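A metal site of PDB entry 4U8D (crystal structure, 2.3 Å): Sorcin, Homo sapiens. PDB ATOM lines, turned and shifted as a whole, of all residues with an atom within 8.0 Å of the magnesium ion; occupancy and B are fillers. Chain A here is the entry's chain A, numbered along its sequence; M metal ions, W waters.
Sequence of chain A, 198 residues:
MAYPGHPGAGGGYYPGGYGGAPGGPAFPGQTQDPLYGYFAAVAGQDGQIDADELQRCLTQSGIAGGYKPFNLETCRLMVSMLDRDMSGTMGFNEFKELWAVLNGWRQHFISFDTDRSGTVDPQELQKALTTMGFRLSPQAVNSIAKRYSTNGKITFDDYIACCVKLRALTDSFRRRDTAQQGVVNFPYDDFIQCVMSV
The backbone NH of Gly 118 is in hydrogen-bond range of the side-chain carboxylate of Asp 113 (2.9 Å).
OG of Ser 117 lies close to O of Thr 119, 2.9 Å away.
O of Asp 113 is in hydrogen-bond range of NH2 of Arg 116, at 2.9 Å.
The magnesium ion is bound by water W1 (1.9 Å), the side-chain hydroxyl of Ser 117 (2.1 Å), the side-chain carboxylate of Asp 115 (2.2 Å) and the side-chain carboxylate of Asp 113 (2.2 Å).
Slightly farther from the magnesium ion lies the backbone carbonyl oxygen (O) of Thr 119 (2.8 Å).
Four residues have an atom within 4 Å of the magnesium ion: Asp 113, Asp 115, Ser 117 and Thr 119.
Along chain A the residues within 4 Å of the magnesium ion span positions 113 to 119.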
ATOM      1  N   TYR A  67     -33.212  22.010   4.676  1.00  0.00           N
ATOM      2  CA  TYR A  67     -32.231  21.233   3.918  1.00  0.00           C
ATOM      3  C   TYR A  67     -32.351  21.481   2.405  1.00  0.00           C
ATOM      4  O   TYR A  67     -33.289  22.129   1.921  1.00  0.00           O
ATOM      5  CB  TYR A  67     -32.348  19.714   4.160  1.00  0.00           C
ATOM      6  CG  TYR A  67     -32.845  19.211   5.519  1.00  0.00           C
ATOM      7  CD1 TYR A  67     -32.435  19.782   6.723  1.00  0.00           C
ATOM      8  CD2 TYR A  67     -33.702  18.095   5.583  1.00  0.00           C
ATOM      9  CE1 TYR A  67     -32.890  19.283   7.955  1.00  0.00           C
ATOM     10  CE2 TYR A  67     -34.152  17.592   6.794  1.00  0.00           C
ATOM     11  CZ  TYR A  67     -33.748  18.180   7.974  1.00  0.00           C
ATOM     12  OH  TYR A  67     -34.208  17.631   9.150  1.00  0.00           O
ATOM     13  N   PHE A 109     -36.569  10.117  10.817  1.00  0.00           N
ATOM     14  CA  PHE A 109     -35.327  10.834  10.590  1.00  0.00           C
ATOM     15  C   PHE A 109     -35.107  11.924  11.618  1.00  0.00           C
ATOM     16  O   PHE A 109     -34.020  12.015  12.176  1.00  0.00           O
ATOM     17  CB  PHE A 109     -35.325  11.442   9.197  1.00  0.00           C
ATOM     18  CG  PHE A 109     -34.045  12.080   8.771  1.00  0.00           C
ATOM     19  CD1 PHE A 109     -33.095  11.364   8.050  1.00  0.00           C
ATOM     20  CD2 PHE A 109     -33.821  13.425   8.991  1.00  0.00           C
ATOM     21  CE1 PHE A 109     -31.922  11.971   7.595  1.00  0.00           C
ATOM     22  CE2 PHE A 109     -32.661  14.036   8.551  1.00  0.00           C
ATOM     23  CZ  PHE A 109     -31.697  13.311   7.844  1.00  0.00           C
ATOM     24  N   ILE A 110     -36.105  12.789  11.840  1.00  0.00           N
ATOM     25  CA  ILE A 110     -35.882  13.953  12.755  1.00  0.00           C
ATOM     26  C   ILE A 110     -35.802  13.552  14.238  1.00  0.00           C
ATOM     27  O   ILE A 110     -35.183  14.277  15.010  1.00  0.00           O
ATOM     28  CB  ILE A 110     -36.846  15.149  12.535  1.00  0.00           C
ATOM     29  CG1 ILE A 110     -38.303  14.766  12.739  1.00  0.00           C
ATOM     30  CG2 ILE A 110     -36.627  15.802  11.165  1.00  0.00           C
ATOM     31  CD1 ILE A 110     -39.248  15.816  12.202  1.00  0.00           C
ATOM     32  N   PHE A 112     -33.766  11.100  15.215  1.00  0.00           N
ATOM     33  CA  PHE A 112     -32.346  10.883  15.379  1.00  0.00           C
ATOM     34  C   PHE A 112     -31.500  11.939  14.693  1.00  0.00           C
ATOM     35  O   PHE A 112     -30.291  11.820  14.704  1.00  0.00           O
ATOM     36  CB  PHE A 112     -31.984   9.517  14.856  1.00  0.00           C
ATOM     37  CG  PHE A 112     -32.793   8.413  15.466  1.00  0.00           C
ATOM     38  CD1 PHE A 112     -32.590   8.050  16.788  1.00  0.00           C
ATOM     39  CD2 PHE A 112     -33.757   7.753  14.731  1.00  0.00           C
ATOM     40  CE1 PHE A 112     -33.350   7.037  17.373  1.00  0.00           C
ATOM     41  CE2 PHE A 112     -34.518   6.748  15.301  1.00  0.00           C
ATOM     42  CZ  PHE A 112     -34.315   6.385  16.622  1.00  0.00           C
ATOM     43  N   ASP A 113     -32.092  12.971  14.111  1.00  0.00           N
ATOM     44  CA  ASP A 113     -31.271  14.107  13.703  1.00  0.00           C
ATOM     45  C   ASP A 113     -31.154  15.007  14.913  1.00  0.00           C
ATOM     46  O   ASP A 113     -31.770  16.091  14.993  1.00  0.00           O
ATOM     47  CB  ASP A 113     -31.826  14.878  12.503  1.00  0.00           C
ATOM     48  CG  ASP A 113     -30.863  15.958  12.004  1.00  0.00           C
ATOM     49  OD1 ASP A 113     -29.667  15.930  12.433  1.00  0.00           O
ATOM     50  OD2 ASP A 113     -31.268  16.822  11.185  1.00  0.00           O
ATOM     51  N   THR A 114     -30.333  14.545  15.860  1.00  0.00           N
ATOM     52  CA  THR A 114     -30.162  15.186  17.162  1.00  0.00           C
ATOM     53  C   THR A 114     -29.498  16.587  17.109  1.00  0.00           C
ATOM     54  O   THR A 114     -29.720  17.390  17.992  1.00  0.00           O
ATOM     55  CB  THR A 114     -29.411  14.259  18.144  1.00  0.00           C
ATOM     56  OG1 THR A 114     -28.416  13.515  17.415  1.00  0.00           O
ATOM     57  CG2 THR A 114     -30.383  13.272  18.824  1.00  0.00           C
ATOM     58  N   ASP A 115     -28.746  16.886  16.037  1.00  0.00           N
ATOM     59  CA  ASP A 115     -28.107  18.214  15.889  1.00  0.00           C
ATOM     60  C   ASP A 115     -28.696  19.104  14.761  1.00  0.00           C
ATOM     61  O   ASP A 115     -28.080  20.102  14.393  1.00  0.00           O
ATOM     62  CB  ASP A 115     -26.571  18.097  15.762  1.00  0.00           C
ATOM     63  CG  ASP A 115     -26.129  16.992  14.789  1.00  0.00           C
ATOM     64  OD1 ASP A 115     -26.714  15.892  14.810  1.00  0.00           O
ATOM     65  OD2 ASP A 115     -25.163  17.231  14.036  1.00  0.00           O
ATOM     66  N   ARG A 116     -29.877  18.756  14.236  1.00  0.00           N
ATOM     67  CA  ARG A 116     -30.590  19.545  13.193  1.00  0.00           C
ATOM     68  C   ARG A 116     -29.765  19.717  11.910  1.00  0.00           C
ATOM     69  O   ARG A 116     -30.069  20.595  11.080  1.00  0.00           O
ATOM     70  CB  ARG A 116     -31.013  20.922  13.728  1.00  0.00           C
ATOM     71  CG  ARG A 116     -32.282  20.913  14.560  1.00  0.00           C
ATOM     72  CD  ARG A 116     -32.095  20.138  15.853  1.00  0.00           C
ATOM     73  NE  ARG A 116     -33.306  19.419  16.213  1.00  0.00           N
ATOM     74  CZ  ARG A 116     -33.344  18.292  16.920  1.00  0.00           C
ATOM     75  NH1 ARG A 116     -34.516  17.726  17.189  1.00  0.00           N
ATOM     76  NH2 ARG A 116     -32.244  17.728  17.368  1.00  0.00           N
ATOM     77  N   SER A 117     -28.763  18.858  11.730  1.00  0.00           N
ATOM     78  CA  SER A 117     -27.833  18.940  10.617  1.00  0.00           C
ATOM     79  C   SER A 117     -28.523  18.864   9.250  1.00  0.00           C
ATOM     80  O   SER A 117     -28.081  19.480   8.281  1.00  0.00           O
ATOM     81  CB  SER A 117     -26.769  17.835  10.734  1.00  0.00           C
ATOM     82  OG  SER A 117     -27.235  16.703  11.468  1.00  0.00           O
ATOM     83  N   GLY A 118     -29.608  18.096   9.182  1.00  0.00           N
ATOM     84  CA  GLY A 118     -30.141  17.644   7.908  1.00  0.00           C
ATOM     85  C   GLY A 118     -29.398  16.413   7.414  1.00  0.00           C
ATOM     86  O   GLY A 118     -29.478  16.066   6.238  1.00  0.00           O
ATOM     87  N   THR A 119     -28.672  15.765   8.334  1.00  0.00           N
ATOM     88  CA  THR A 119     -27.884  14.592   8.050  1.00  0.00           C
ATOM     89  C   THR A 119     -27.943  13.703   9.246  1.00  0.00           C
ATOM     90  O   THR A 119     -28.085  14.166  10.375  1.00  0.00           O
ATOM     91  CB  THR A 119     -26.385  14.905   7.767  1.00  0.00           C
ATOM     92  OG1 THR A 119     -25.722  15.298   8.980  1.00  0.00           O
ATOM     93  CG2 THR A 119     -26.211  15.972   6.697  1.00  0.00           C
ATOM     94  N   VAL A 120     -27.845  12.411   9.002  1.00  0.00           N
ATOM     95  CA  VAL A 120     -27.698  11.429  10.064  1.00  0.00           C
ATOM     96  C   VAL A 120     -26.430  10.611   9.803  1.00  0.00           C
ATOM     97  O   VAL A 120     -25.940  10.548   8.667  1.00  0.00           O
ATOM     98  CB  VAL A 120     -28.948  10.515  10.207  1.00  0.00           C
ATOM     99  CG1 VAL A 120     -30.165  11.326  10.594  1.00  0.00           C
ATOM    100  CG2 VAL A 120     -29.218   9.728   8.929  1.00  0.00           C
ATOM    101  N   ASP A 121     -25.863  10.038  10.849  1.00  0.00           N
ATOM    102  CA  ASP A 121     -24.685   9.240  10.693  1.00  0.00           C
ATOM    103  C   ASP A 121     -25.200   7.832  10.647  1.00  0.00           C
ATOM    104  O   ASP A 121     -26.400   7.629  10.856  1.00  0.00           O
ATOM    105  CB  ASP A 121     -23.655   9.486  11.830  1.00  0.00           C
ATOM    106  CG  ASP A 121     -24.081   8.890  13.182  1.00  0.00           C
ATOM    107  OD1 ASP A 121     -24.643   7.775  13.254  1.00  0.00           O
ATOM    108  OD2 ASP A 121     -23.819   9.555  14.205  1.00  0.00           O
ATOM    109  N   GLU A 124     -27.356   6.478  13.715  1.00  0.00           N
ATOM    110  CA  GLU A 124     -28.655   7.139  13.687  1.00  0.00           C
ATOM    111  C   GLU A 124     -29.536   6.490  12.591  1.00  0.00           C
ATOM    112  O   GLU A 124     -30.660   6.051  12.865  1.00  0.00           O
ATOM    113  CB  GLU A 124     -28.453   8.640  13.469  1.00  0.00           C
ATOM    114  CG  GLU A 124     -27.788   9.327  14.666  1.00  0.00           C
ATOM    115  CD  GLU A 124     -27.270  10.721  14.384  1.00  0.00           C
ATOM    116  OE1 GLU A 124     -27.226  11.546  15.325  1.00  0.00           O
ATOM    117  OE2 GLU A 124     -26.899  11.010  13.234  1.00  0.00           O
ATOM    118  N   LYS A 153     -21.677  11.229   6.313  1.00  0.00           N
ATOM    119  CA  LYS A 153     -23.028  11.468   6.778  1.00  0.00           C
ATOM    120  C   LYS A 153     -24.002  11.406   5.623  1.00  0.00           C
ATOM    121  O   LYS A 153     -23.641  11.709   4.487  1.00  0.00           O
ATOM    122  CB  LYS A 153     -23.092  12.806   7.508  1.00  0.00           C
ATOM    123  CG  LYS A 153     -22.745  12.652   8.985  1.00  0.00           C
ATOM    124  CD  LYS A 153     -22.176  13.927   9.571  1.00  0.00           C
ATOM    125  CE  LYS A 153     -21.648  13.641  10.958  1.00  0.00           C
ATOM    126  NZ  LYS A 153     -20.601  14.636  11.318  1.00  0.00           N
ATOM    127  N   ILE A 154     -25.230  10.976   5.927  1.00  0.00           N
ATOM    128  CA  ILE A 154     -26.307  10.830   4.923  1.00  0.00           C
ATOM    129  C   ILE A 154     -27.295  11.997   4.933  1.00  0.00           C
ATOM    130  O   ILE A 154     -27.948  12.233   5.922  1.00  0.00           O
ATOM    131  CB  ILE A 154     -27.126   9.546   5.174  1.00  0.00           C
ATOM    132  CG1 ILE A 154     -26.210   8.327   5.158  1.00  0.00           C
ATOM    133  CG2 ILE A 154     -28.228   9.388   4.139  1.00  0.00           C
ATOM    134  CD1 ILE A 154     -25.873   7.824   6.553  1.00  0.00           C
HETATM  135 MG    MG M   1     -27.638  15.282  12.928  1.00  0.00          MG
HETATM  136  O   HOH W   1     -27.101  13.821  13.962  1.00  0.00           O
